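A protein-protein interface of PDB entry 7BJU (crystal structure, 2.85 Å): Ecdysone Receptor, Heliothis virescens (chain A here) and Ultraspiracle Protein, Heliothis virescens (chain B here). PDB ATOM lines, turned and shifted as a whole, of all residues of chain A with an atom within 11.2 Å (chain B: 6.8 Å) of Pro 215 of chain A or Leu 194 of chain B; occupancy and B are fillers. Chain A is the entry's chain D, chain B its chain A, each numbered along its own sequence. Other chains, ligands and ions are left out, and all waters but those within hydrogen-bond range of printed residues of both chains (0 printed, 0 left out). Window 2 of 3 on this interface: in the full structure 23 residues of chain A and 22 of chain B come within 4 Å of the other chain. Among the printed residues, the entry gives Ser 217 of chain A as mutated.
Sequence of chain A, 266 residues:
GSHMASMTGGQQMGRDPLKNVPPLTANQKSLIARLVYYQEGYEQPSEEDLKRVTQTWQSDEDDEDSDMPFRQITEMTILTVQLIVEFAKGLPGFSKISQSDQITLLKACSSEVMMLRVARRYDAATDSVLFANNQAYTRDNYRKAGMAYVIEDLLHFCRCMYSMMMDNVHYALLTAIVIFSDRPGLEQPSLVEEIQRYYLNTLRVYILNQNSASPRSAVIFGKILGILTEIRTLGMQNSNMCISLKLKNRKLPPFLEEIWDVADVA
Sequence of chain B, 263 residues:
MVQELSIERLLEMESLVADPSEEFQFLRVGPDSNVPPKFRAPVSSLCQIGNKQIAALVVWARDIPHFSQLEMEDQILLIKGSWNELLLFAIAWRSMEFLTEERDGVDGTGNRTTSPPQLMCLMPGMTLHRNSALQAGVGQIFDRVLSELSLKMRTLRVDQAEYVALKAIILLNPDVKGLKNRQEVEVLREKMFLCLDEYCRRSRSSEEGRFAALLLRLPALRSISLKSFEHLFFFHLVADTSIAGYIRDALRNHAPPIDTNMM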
ATOM      1  N   ASN A  20     -17.022  -4.729 -15.237  1.00  0.00           N
ATOM      2  CA  ASN A  20     -17.588  -4.568 -16.570  1.00  0.00           C
ATOM      3  C   ASN A  20     -17.043  -5.636 -17.512  1.00  0.00           C
ATOM      4  O   ASN A  20     -17.629  -6.709 -17.660  1.00  0.00           O
ATOM      5  CB  ASN A  20     -17.283  -3.173 -17.121  1.00  0.00           C
ATOM      6  CG  ASN A  20     -18.268  -2.737 -18.193  1.00  0.00           C
ATOM      7  OD1 ASN A  20     -18.357  -1.554 -18.522  1.00  0.00           O
ATOM      8  ND2 ASN A  20     -19.022  -3.688 -18.732  1.00  0.00           N
ATOM      9  N   VAL A  21     -15.921  -5.332 -18.149  1.00  0.00           N
ATOM     10  CA  VAL A  21     -15.252  -6.234 -19.082  1.00  0.00           C
ATOM     11  C   VAL A  21     -13.924  -6.647 -18.458  1.00  0.00           C
ATOM     12  O   VAL A  21     -13.115  -5.775 -18.112  1.00  0.00           O
ATOM     13  CB  VAL A  21     -15.037  -5.574 -20.454  1.00  0.00           C
ATOM     14  CG1 VAL A  21     -14.598  -6.609 -21.476  1.00  0.00           C
ATOM     15  CG2 VAL A  21     -16.307  -4.867 -20.908  1.00  0.00           C
ATOM     16  N   ARG A 204      -9.761 -15.392 -25.977  1.00  0.00           N
ATOM     17  CA  ARG A 204     -11.121 -15.076 -25.548  1.00  0.00           C
ATOM     18  C   ARG A 204     -11.185 -13.699 -24.900  1.00  0.00           C
ATOM     19  O   ARG A 204     -12.071 -12.893 -25.210  1.00  0.00           O
ATOM     20  CB  ARG A 204     -11.625 -16.148 -24.582  1.00  0.00           C
ATOM     21  CG  ARG A 204     -13.050 -15.931 -24.089  1.00  0.00           C
ATOM     22  CD  ARG A 204     -13.388 -16.888 -22.957  1.00  0.00           C
ATOM     23  NE  ARG A 204     -12.568 -16.638 -21.777  1.00  0.00           N
ATOM     24  CZ  ARG A 204     -12.934 -15.868 -20.761  1.00  0.00           C
ATOM     25  NH1 ARG A 204     -14.111 -15.263 -20.740  1.00  0.00           N
ATOM     26  NH2 ARG A 204     -12.098 -15.701 -19.741  1.00  0.00           N
ATOM     27  N   ILE A 207     -10.716 -10.803 -27.483  1.00  0.00           N
ATOM     28  CA  ILE A 207     -11.937 -10.532 -28.236  1.00  0.00           C
ATOM     29  C   ILE A 207     -12.965  -9.834 -27.353  1.00  0.00           C
ATOM     30  O   ILE A 207     -13.654  -8.904 -27.792  1.00  0.00           O
ATOM     31  CB  ILE A 207     -12.493 -11.842 -28.830  1.00  0.00           C
ATOM     32  CG1 ILE A 207     -11.508 -12.429 -29.844  1.00  0.00           C
ATOM     33  CG2 ILE A 207     -13.857 -11.610 -29.465  1.00  0.00           C
ATOM     34  CD1 ILE A 207     -11.866 -13.825 -30.315  1.00  0.00           C
ATOM     35  N   LEU A 208     -13.086 -10.271 -26.098  1.00  0.00           N
ATOM     36  CA  LEU A 208     -14.045  -9.660 -25.181  1.00  0.00           C
ATOM     37  C   LEU A 208     -13.729  -8.185 -24.953  1.00  0.00           C
ATOM     38  O   LEU A 208     -14.622  -7.333 -25.010  1.00  0.00           O
ATOM     39  CB  LEU A 208     -14.057 -10.420 -23.854  1.00  0.00           C
ATOM     40  CG  LEU A 208     -14.962 -11.651 -23.780  1.00  0.00           C
ATOM     41  CD1 LEU A 208     -14.739 -12.403 -22.479  1.00  0.00           C
ATOM     42  CD2 LEU A 208     -16.416 -11.237 -23.912  1.00  0.00           C
ATOM     43  N   ASN A 209     -12.459  -7.866 -24.690  1.00  0.00           N
ATOM     44  CA  ASN A 209     -12.084  -6.473 -24.473  1.00  0.00           C
ATOM     45  C   ASN A 209     -12.215  -5.647 -25.745  1.00  0.00           C
ATOM     46  O   ASN A 209     -12.546  -4.458 -25.680  1.00  0.00           O
ATOM     47  CB  ASN A 209     -10.656  -6.386 -23.934  1.00  0.00           C
ATOM     48  CG  ASN A 209     -10.579  -6.665 -22.447  1.00  0.00           C
ATOM     49  OD1 ASN A 209     -11.394  -6.171 -21.668  1.00  0.00           O
ATOM     50  ND2 ASN A 209      -9.597  -7.460 -22.045  1.00  0.00           N
ATOM     51  N   GLN A 210     -11.962  -6.252 -26.905  1.00  0.00           N
ATOM     52  CA  GLN A 210     -12.094  -5.537 -28.167  1.00  0.00           C
ATOM     53  C   GLN A 210     -13.545  -5.332 -28.578  1.00  0.00           C
ATOM     54  O   GLN A 210     -13.807  -4.519 -29.471  1.00  0.00           O
ATOM     55  CB  GLN A 210     -11.340  -6.282 -29.270  1.00  0.00           C
ATOM     56  CG  GLN A 210     -10.365  -5.414 -30.055  1.00  0.00           C
ATOM     57  CD  GLN A 210      -9.266  -4.827 -29.183  1.00  0.00           C
ATOM     58  OE1 GLN A 210      -8.976  -5.333 -28.099  1.00  0.00           O
ATOM     59  NE2 GLN A 210      -8.650  -3.751 -29.659  1.00  0.00           N
ATOM     60  N   ASN A 211     -14.488  -6.037 -27.953  1.00  0.00           N
ATOM     61  CA  ASN A 211     -15.902  -5.909 -28.282  1.00  0.00           C
ATOM     62  C   ASN A 211     -16.749  -5.456 -27.099  1.00  0.00           C
ATOM     63  O   ASN A 211     -17.981  -5.517 -27.178  1.00  0.00           O
ATOM     64  CB  ASN A 211     -16.442  -7.233 -28.832  1.00  0.00           C
ATOM     65  CG  ASN A 211     -15.892  -7.560 -30.205  1.00  0.00           C
ATOM     66  OD1 ASN A 211     -16.420  -7.110 -31.222  1.00  0.00           O
ATOM     67  ND2 ASN A 211     -14.822  -8.347 -30.243  1.00  0.00           N
ATOM     68  N   SER A 212     -16.124  -5.001 -26.009  1.00  0.00           N
ATOM     69  CA  SER A 212     -16.841  -4.501 -24.831  1.00  0.00           C
ATOM     70  C   SER A 212     -17.800  -5.549 -24.271  1.00  0.00           C
ATOM     71  O   SER A 212     -18.941  -5.246 -23.916  1.00  0.00           O
ATOM     72  CB  SER A 212     -17.584  -3.199 -25.145  1.00  0.00           C
ATOM     73  OG  SER A 212     -16.695  -2.205 -25.621  1.00  0.00           O
ATOM     74  N   ALA A 213     -17.330  -6.796 -24.197  1.00  0.00           N
ATOM     75  CA  ALA A 213     -18.115  -7.923 -23.686  1.00  0.00           C
ATOM     76  C   ALA A 213     -19.424  -8.103 -24.450  1.00  0.00           C
ATOM     77  O   ALA A 213     -20.422  -8.566 -23.891  1.00  0.00           O
ATOM     78  CB  ALA A 213     -18.389  -7.779 -22.185  1.00  0.00           C
ATOM     79  N   SER A 214     -19.431  -7.739 -25.731  1.00  0.00           N
ATOM     80  CA  SER A 214     -20.616  -7.925 -26.551  1.00  0.00           C
ATOM     81  C   SER A 214     -20.911  -9.415 -26.714  1.00  0.00           C
ATOM     82  O   SER A 214     -19.994 -10.242 -26.710  1.00  0.00           O
ATOM     83  CB  SER A 214     -20.425  -7.277 -27.922  1.00  0.00           C
ATOM     84  OG  SER A 214     -21.478  -7.612 -28.808  1.00  0.00           O
ATOM     85  N   PRO A 215     -22.187  -9.788 -26.842  1.00  0.00           N
ATOM     86  CA  PRO A 215     -22.507 -11.201 -27.102  1.00  0.00           C
ATOM     87  C   PRO A 215     -21.850 -11.739 -28.360  1.00  0.00           C
ATOM     88  O   PRO A 215     -21.609 -12.950 -28.456  1.00  0.00           O
ATOM     89  CB  PRO A 215     -24.038 -11.196 -27.218  1.00  0.00           C
ATOM     90  CG  PRO A 215     -24.472  -9.992 -26.450  1.00  0.00           C
ATOM     91  CD  PRO A 215     -23.397  -8.967 -26.659  1.00  0.00           C
ATOM     92  N   ARG A 216     -21.534 -10.869 -29.322  1.00  0.00           N
ATOM     93  CA  ARG A 216     -20.862 -11.275 -30.550  1.00  0.00           C
ATOM     94  C   ARG A 216     -19.434 -11.752 -30.321  1.00  0.00           C
ATOM     95  O   ARG A 216     -18.807 -12.241 -31.267  1.00  0.00           O
ATOM     96  CB  ARG A 216     -20.867 -10.118 -31.549  1.00  0.00           C
ATOM     97  CG  ARG A 216     -22.160  -9.988 -32.335  1.00  0.00           C
ATOM     98  CD  ARG A 216     -22.011 -10.603 -33.714  1.00  0.00           C
ATOM     99  NE  ARG A 216     -23.200 -11.342 -34.122  1.00  0.00           N
ATOM    100  CZ  ARG A 216     -23.321 -11.984 -35.276  1.00  0.00           C
ATOM    101  NH1 ARG A 216     -22.349 -11.978 -36.175  1.00  0.00           N
ATOM    102  NH2 ARG A 216     -24.443 -12.648 -35.535  1.00  0.00           N
ATOM    103  N   SER A 217     -18.905 -11.617 -29.101  1.00  0.00           N
ATOM    104  CA  SER A 217     -17.578 -12.148 -28.810  1.00  0.00           C
ATOM    105  C   SER A 217     -17.540 -13.657 -29.011  1.00  0.00           C
ATOM    106  O   SER A 217     -16.541 -14.204 -29.494  1.00  0.00           O
ATOM    107  CB  SER A 217     -17.174 -11.790 -27.381  1.00  0.00           C
ATOM    108  OG  SER A 217     -17.291 -10.397 -27.147  1.00  0.00           O
ATOM    109  N   ALA A 218     -18.624 -14.346 -28.645  1.00  0.00           N
ATOM    110  CA  ALA A 218     -18.688 -15.789 -28.840  1.00  0.00           C
ATOM    111  C   ALA A 218     -18.681 -16.146 -30.321  1.00  0.00           C
ATOM    112  O   ALA A 218     -18.114 -17.172 -30.716  1.00  0.00           O
ATOM    113  CB  ALA A 218     -19.935 -16.354 -28.164  1.00  0.00           C
ATOM    114  N   VAL A 219     -19.317 -15.318 -31.151  1.00  0.00           N
ATOM    115  CA  VAL A 219     -19.342 -15.572 -32.587  1.00  0.00           C
ATOM    116  C   VAL A 219     -17.941 -15.447 -33.175  1.00  0.00           C
ATOM    117  O   VAL A 219     -17.470 -16.336 -33.896  1.00  0.00           O
ATOM    118  CB  VAL A 219     -20.331 -14.620 -33.281  1.00  0.00           C
ATOM    119  CG1 VAL A 219     -20.254 -14.795 -34.783  1.00  0.00           C
ATOM    120  CG2 VAL A 219     -21.745 -14.869 -32.776  1.00  0.00           C
ATOM    121  N   ILE A 220     -17.255 -14.344 -32.873  1.00  0.00           N
ATOM    122  CA  ILE A 220     -15.883 -14.160 -33.343  1.00  0.00           C
ATOM    123  C   ILE A 220     -14.994 -15.284 -32.827  1.00  0.00           C
ATOM    124  O   ILE A 220     -14.212 -15.879 -33.578  1.00  0.00           O
ATOM    125  CB  ILE A 220     -15.354 -12.780 -32.914  1.00  0.00           C
ATOM    126  CG1 ILE A 220     -16.143 -11.664 -33.605  1.00  0.00           C
ATOM    127  CG2 ILE A 220     -13.863 -12.665 -33.205  1.00  0.00           C
ATOM    128  CD1 ILE A 220     -15.853 -10.279 -33.060  1.00  0.00           C
ATOM    129  N   PHE A 221     -15.108 -15.594 -31.533  1.00  0.00           N
ATOM    130  CA  PHE A 221     -14.306 -16.659 -30.939  1.00  0.00           C
ATOM    131  C   PHE A 221     -14.622 -18.005 -31.580  1.00  0.00           C
ATOM    132  O   PHE A 221     -13.714 -18.764 -31.942  1.00  0.00           O
ATOM    133  CB  PHE A 221     -14.555 -16.709 -29.432  1.00  0.00           C
ATOM    134  CG  PHE A 221     -13.513 -17.469 -28.664  1.00  0.00           C
ATOM    135  CD1 PHE A 221     -12.232 -17.625 -29.168  1.00  0.00           C
ATOM    136  CD2 PHE A 221     -13.818 -18.028 -27.434  1.00  0.00           C
ATOM    137  CE1 PHE A 221     -11.275 -18.325 -28.455  1.00  0.00           C
ATOM    138  CE2 PHE A 221     -12.867 -18.728 -26.718  1.00  0.00           C
ATOM    139  CZ  PHE A 221     -11.593 -18.878 -27.228  1.00  0.00           C
ATOM    140  N   GLY A 222     -15.911 -18.317 -31.732  1.00  0.00           N
ATOM    141  CA  GLY A 222     -16.292 -19.612 -32.271  1.00  0.00           C
ATOM    142  C   GLY A 222     -15.857 -19.801 -33.711  1.00  0.00           C
ATOM    143  O   GLY A 222     -15.435 -20.892 -34.103  1.00  0.00           O
ATOM    144  N   LYS A 223     -15.955 -18.743 -34.521  1.00  0.00           N
ATOM    145  CA  LYS A 223     -15.537 -18.843 -35.915  1.00  0.00           C
ATOM    146  C   LYS A 223     -14.040 -19.100 -36.029  1.00  0.00           C
ATOM    147  O   LYS A 223     -13.601 -19.861 -36.901  1.00  0.00           O
ATOM    148  CB  LYS A 223     -15.927 -17.576 -36.677  1.00  0.00           C
ATOM    149  CG  LYS A 223     -17.425 -17.410 -36.874  1.00  0.00           C
ATOM    150  CD  LYS A 223     -17.752 -16.589 -38.113  1.00  0.00           C
ATOM    151  CE  LYS A 223     -17.298 -15.148 -37.981  1.00  0.00           C
ATOM    152  NZ  LYS A 223     -17.690 -14.342 -39.174  1.00  0.00           N
ATOM    153  N   ILE B   7     -31.425 -24.070 -28.309  1.00  0.00           N
ATOM    154  CA  ILE B   7     -31.040 -25.355 -27.733  1.00  0.00           C
ATOM    155  C   ILE B   7     -32.266 -26.097 -27.219  1.00  0.00           C
ATOM    156  O   ILE B   7     -32.324 -27.332 -27.267  1.00  0.00           O
ATOM    157  CB  ILE B   7     -29.991 -25.145 -26.621  1.00  0.00           C
ATOM    158  CG1 ILE B   7     -28.753 -24.433 -27.177  1.00  0.00           C
ATOM    159  CG2 ILE B   7     -29.606 -26.471 -25.983  1.00  0.00           C
ATOM    160  CD1 ILE B   7     -27.628 -24.279 -26.178  1.00  0.00           C
ATOM    161  N   ARG B 189     -25.301 -20.686 -38.067  1.00  0.00           N
ATOM    162  CA  ARG B 189     -24.235 -21.148 -37.180  1.00  0.00           C
ATOM    163  C   ARG B 189     -23.900 -20.102 -36.125  1.00  0.00           C
ATOM    164  O   ARG B 189     -23.670 -20.442 -34.959  1.00  0.00           O
ATOM    165  CB  ARG B 189     -22.983 -21.510 -37.978  1.00  0.00           C
ATOM    166  CG  ARG B 189     -21.768 -21.765 -37.090  1.00  0.00           C
ATOM    167  CD  ARG B 189     -20.537 -22.166 -37.879  1.00  0.00           C
ATOM    168  NE  ARG B 189     -20.420 -23.613 -38.018  1.00  0.00           N
ATOM    169  CZ  ARG B 189     -19.319 -24.238 -38.415  1.00  0.00           C
ATOM    170  NH1 ARG B 189     -18.216 -23.572 -38.715  1.00  0.00           N
ATOM    171  NH2 ARG B 189     -19.325 -25.565 -38.508  1.00  0.00           N
ATOM    172  N   GLU B 190     -23.870 -18.824 -36.514  1.00  0.00           N
ATOM    173  CA  GLU B 190     -23.556 -17.773 -35.552  1.00  0.00           C
ATOM    174  C   GLU B 190     -24.611 -17.690 -34.457  1.00  0.00           C
ATOM    175  O   GLU B 190     -24.289 -17.374 -33.306  1.00  0.00           O
ATOM    176  CB  GLU B 190     -23.410 -16.433 -36.271  1.00  0.00           C
ATOM    177  CG  GLU B 190     -22.238 -16.386 -37.239  1.00  0.00           C
ATOM    178  CD  GLU B 190     -22.136 -15.070 -37.982  1.00  0.00           C
ATOM    179  OE1 GLU B 190     -23.086 -14.259 -37.899  1.00  0.00           O
ATOM    180  OE2 GLU B 190     -21.103 -14.848 -38.649  1.00  0.00           O
ATOM    181  N   LYS B 191     -25.872 -17.972 -34.791  1.00  0.00           N
ATOM    182  CA  LYS B 191     -26.897 -18.057 -33.758  1.00  0.00           C
ATOM    183  C   LYS B 191     -26.622 -19.210 -32.804  1.00  0.00           C
ATOM    184  O   LYS B 191     -26.917 -19.111 -31.607  1.00  0.00           O
ATOM    185  CB  LYS B 191     -28.279 -18.210 -34.394  1.00  0.00           C
ATOM    186  CG  LYS B 191     -29.422 -18.270 -33.389  1.00  0.00           C
ATOM    187  CD  LYS B 191     -29.480 -17.008 -32.545  1.00  0.00           C
ATOM    188  CE  LYS B 191     -30.428 -17.169 -31.368  1.00  0.00           C
ATOM    189  NZ  LYS B 191     -31.813 -17.506 -31.791  1.00  0.00           N
ATOM    190  N   MET B 192     -26.050 -20.306 -33.310  1.00  0.00           N
ATOM    191  CA  MET B 192     -25.738 -21.439 -32.447  1.00  0.00           C
ATOM    192  C   MET B 192     -24.576 -21.124 -31.514  1.00  0.00           C
ATOM    193  O   MET B 192     -24.558 -21.575 -30.363  1.00  0.00           O
ATOM    194  CB  MET B 192     -25.432 -22.675 -33.292  1.00  0.00           C
ATOM    195  CG  MET B 192     -26.646 -23.260 -33.987  1.00  0.00           C
ATOM    196  SD  MET B 192     -27.979 -23.623 -32.831  1.00  0.00           S
ATOM    197  CE  MET B 192     -27.131 -24.661 -31.641  1.00  0.00           C
ATOM    198  N   PHE B 193     -23.591 -20.358 -31.993  1.00  0.00           N
ATOM    199  CA  PHE B 193     -22.522 -19.899 -31.112  1.00  0.00           C
ATOM    200  C   PHE B 193     -23.082 -19.075 -29.960  1.00  0.00           C
ATOM    201  O   PHE B 193     -22.654 -19.227 -28.810  1.00  0.00           O
ATOM    202  CB  PHE B 193     -21.499 -19.085 -31.905  1.00  0.00           C
ATOM    203  CG  PHE B 193     -20.606 -19.915 -32.781  1.00  0.00           C
ATOM    204  CD1 PHE B 193     -20.176 -21.166 -32.372  1.00  0.00           C
ATOM    205  CD2 PHE B 193     -20.194 -19.440 -34.016  1.00  0.00           C
ATOM    206  CE1 PHE B 193     -19.349 -21.929 -33.178  1.00  0.00           C
ATOM    207  CE2 PHE B 193     -19.369 -20.197 -34.827  1.00  0.00           C
ATOM    208  CZ  PHE B 193     -18.946 -21.444 -34.407  1.00  0.00           C
ATOM    209  N   LEU B 194     -24.045 -18.196 -30.254  1.00  0.00           N
ATOM    210  CA  LEU B 194     -24.688 -17.415 -29.203  1.00  0.00           C
ATOM    211  C   LEU B 194     -25.435 -18.313 -28.226  1.00  0.00           C
ATOM    212  O   LEU B 194     -25.357 -18.117 -27.008  1.00  0.00           O
ATOM    213  CB  LEU B 194     -25.643 -16.392 -29.821  1.00  0.00           C
ATOM    214  CG  LEU B 194     -25.023 -15.259 -30.639  1.00  0.00           C
ATOM    215  CD1 LEU B 194     -26.102 -14.479 -31.370  1.00  0.00           C
ATOM    216  CD2 LEU B 194     -24.218 -14.342 -29.738  1.00  0.00           C
ATOM    217  N   CYS B 195     -26.166 -19.306 -28.742  1.00  0.00           N
ATOM    218  CA  CYS B 195     -26.918 -20.202 -27.869  1.00  0.00           C
ATOM    219  C   CYS B 195     -25.990 -21.015 -26.975  1.00  0.00           C
ATOM    220  O   CYS B 195     -26.248 -21.164 -25.775  1.00  0.00           O
ATOM    221  CB  CYS B 195     -27.805 -21.130 -28.702  1.00  0.00           C
ATOM    222  SG  CYS B 195     -29.137 -20.307 -29.612  1.00  0.00           S
ATOM    223  N   LEU B 196     -24.900 -21.542 -27.540  1.00  0.00           N
ATOM    224  CA  LEU B 196     -23.988 -22.371 -26.758  1.00  0.00           C
ATOM    225  C   LEU B 196     -23.264 -21.553 -25.697  1.00  0.00           C
ATOM    226  O   LEU B 196     -23.081 -22.018 -24.566  1.00  0.00           O
ATOM    227  CB  LEU B 196     -22.984 -23.062 -27.680  1.00  0.00           C
ATOM    228  CG  LEU B 196     -22.013 -24.033 -27.003  1.00  0.00           C
ATOM    229  CD1 LEU B 196     -22.775 -25.114 -26.251  1.00  0.00           C
ATOM    230  CD2 LEU B 196     -21.071 -24.648 -28.025  1.00  0.00           C
ATOM    231  N   ASP B 197     -22.841 -20.335 -26.042  1.00  0.00           N
ATOM    232  CA  ASP B 197     -22.158 -19.493 -25.066  1.00  0.00           C
ATOM    233  C   ASP B 197     -23.097 -19.084 -23.940  1.00  0.00           C
ATOM    234  O   ASP B 197     -22.703 -19.076 -22.768  1.00  0.00           O
ATOM    235  CB  ASP B 197     -21.576 -18.263 -25.754  1.00  0.00           C
ATOM    236  CG  ASP B 197     -20.700 -17.440 -24.832  1.00  0.00           C
ATOM    237  OD1 ASP B 197     -19.662 -17.962 -24.377  1.00  0.00           O
ATOM    238  OD2 ASP B 197     -21.048 -16.270 -24.567  1.00  0.00           O
ATOM    239  N   GLU B 198     -24.345 -18.745 -24.276  1.00  0.00           N
ATOM    240  CA  GLU B 198     -25.313 -18.374 -23.249  1.00  0.00           C
ATOM    241  C   GLU B 198     -25.607 -19.544 -22.320  1.00  0.00           C
ATOM    242  O   GLU B 198     -25.704 -19.367 -21.099  1.00  0.00           O
ATOM    243  CB  GLU B 198     -26.600 -17.872 -23.897  1.00  0.00           C
ATOM    244  CG  GLU B 198     -27.710 -17.565 -22.905  1.00  0.00           C
ATOM    245  CD  GLU B 198     -29.057 -17.398 -23.577  1.00  0.00           C
ATOM    246  OE1 GLU B 198     -29.110 -17.460 -24.824  1.00  0.00           O
ATOM    247  OE2 GLU B 198     -30.064 -17.213 -22.862  1.00  0.00           O
ATOM    248  N   TYR B 199     -25.757 -20.749 -22.878  1.00  0.00           N
ATOM    249  CA  TYR B 199     -26.022 -21.915 -22.042  1.00  0.00           C
ATOM    250  C   TYR B 199     -24.864 -22.185 -21.091  1.00  0.00           C
ATOM    251  O   TYR B 199     -25.075 -22.589 -19.942  1.00  0.00           O
ATOM    252  CB  TYR B 199     -26.292 -23.145 -22.909  1.00  0.00           C
ATOM    253  CG  TYR B 199     -26.500 -24.406 -22.098  1.00  0.00           C
ATOM    254  CD1 TYR B 199     -27.733 -24.691 -21.530  1.00  0.00           C
ATOM    255  CD2 TYR B 199     -25.459 -25.302 -21.889  1.00  0.00           C
ATOM    256  CE1 TYR B 199     -27.928 -25.836 -20.781  1.00  0.00           C
ATOM    257  CE2 TYR B 199     -25.644 -26.449 -21.141  1.00  0.00           C
ATOM    258  CZ  TYR B 199     -26.881 -26.710 -20.589  1.00  0.00           C
ATOM    259  OH  TYR B 199     -27.072 -27.854 -19.846  1.00  0.00           O
ATOM    260  N   ARG B 201     -22.910 -19.912 -19.849  1.00  0.00           N
ATOM    261  CA  ARG B 201     -22.860 -18.841 -18.858  1.00  0.00           C
ATOM    262  C   ARG B 201     -23.987 -18.941 -17.838  1.00  0.00           C
ATOM    263  O   ARG B 201     -23.818 -18.521 -16.687  1.00  0.00           O
ATOM    264  CB  ARG B 201     -22.925 -17.474 -19.541  1.00  0.00           C
ATOM    265  CG  ARG B 201     -21.753 -17.138 -20.447  1.00  0.00           C
ATOM    266  CD  ARG B 201     -21.777 -15.658 -20.804  1.00  0.00           C
ATOM    267  NE  ARG B 201     -23.142 -15.151 -20.906  1.00  0.00           N
ATOM    268  CZ  ARG B 201     -23.801 -14.987 -22.045  1.00  0.00           C
ATOM    269  NH1 ARG B 201     -23.241 -15.258 -23.212  1.00  0.00           N
ATOM    270  NH2 ARG B 201     -25.052 -14.537 -22.011  1.00  0.00           N
ATOM    271  N   PHE B 211     -16.735 -23.165 -23.262  1.00  0.00           N
ATOM    272  CA  PHE B 211     -17.126 -22.901 -24.644  1.00  0.00           C
ATOM    273  C   PHE B 211     -16.038 -23.344 -25.614  1.00  0.00           C
ATOM    274  O   PHE B 211     -16.316 -24.003 -26.624  1.00  0.00           O
ATOM    275  CB  PHE B 211     -17.434 -21.412 -24.813  1.00  0.00           C
ATOM    276  CG  PHE B 211     -17.956 -21.044 -26.172  1.00  0.00           C
ATOM    277  CD1 PHE B 211     -19.276 -21.289 -26.511  1.00  0.00           C
ATOM    278  CD2 PHE B 211     -17.131 -20.435 -27.104  1.00  0.00           C
ATOM    279  CE1 PHE B 211     -19.763 -20.947 -27.759  1.00  0.00           C
ATOM    280  CE2 PHE B 211     -17.612 -20.087 -28.354  1.00  0.00           C
ATOM    281  CZ  PHE B 211     -18.930 -20.345 -28.682  1.00  0.00           C
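Of the 20 printed residues of chain A, 6 touch a printed residue of chain B.
Hydrophobic or aromatic side chains of chain B within 4 Å of the printed part of chain A: Phe 193, Leu 194 and Phe 211.
Among the printed residues, 9 pairs touch across the chains.
Pro 215 of chain A touches one residue of chain B.
Leu 194 of chain B touches just these residues of chain A: Pro 215 (3.2 Å) and Val 219 (3.9 Å).
No residue of chain A comes within 4 Å of Lys 191 of chain B.
Cys 195 of chain B touches none of the printed residues of chain A.
Asp 197 of chain B touches one residue of chain A.
Of the printed residues of chain A, Phe 193 of chain B touches Gly 222 and Lys 223.
Of the printed residues of chain A, Glu 190 of chain B touches Arg 216, Val 219 and Lys 223.
Of the printed residues of chain B, Ala 218 of chain A touches Asp 197 and Phe 211.
Asn 209 of chain A touches none of the printed residues of chain B.
Met 192 of chain B touches none of the printed residues of chain A.
The nearest residue of chain B that does not touch Pro 215 of chain A is Asp 197 of chain B (5.1 Å).
The guanidinium group (NH1) of Arg 201 of chain B lies within salt-bridge range of the side-chain carboxylate (OD2) of Asp 197 of chain B, 2.8 Å away.
The side-chain hydroxyl of Ser 214 of chain A lies close to the backbone NH of Arg 216 of chain A, at 3.3 Å.
The side-chain carboxylate (OE1) of Glu 190 of chain B lies within salt-bridge range of the guanidinium group (NH1) of Arg 216 of chain A, at 3.0 Å.
NZ of Lys 223 of chain A lies within salt-bridge range of OE2 of Glu 190 of chain B.
Pro 215 of chain A touches Leu 194 of chain B.
Asp 197 of chain B touches Ala 218 of chain A.
Ala 218 of chain A touches Phe 211 of chain B.
Glu 190 of chain B touches Val 219 of chain A.
Leu 194 of chain B touches Val 219 of chain A (CG to CG2, 3.9 Å).
Gly 222 of chain A touches Phe 193 of chain B (O to CZ, 3.6 Å).
Lys 223 of chain A touches Phe 193 of chain B (N to CE2, 3.7 Å).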
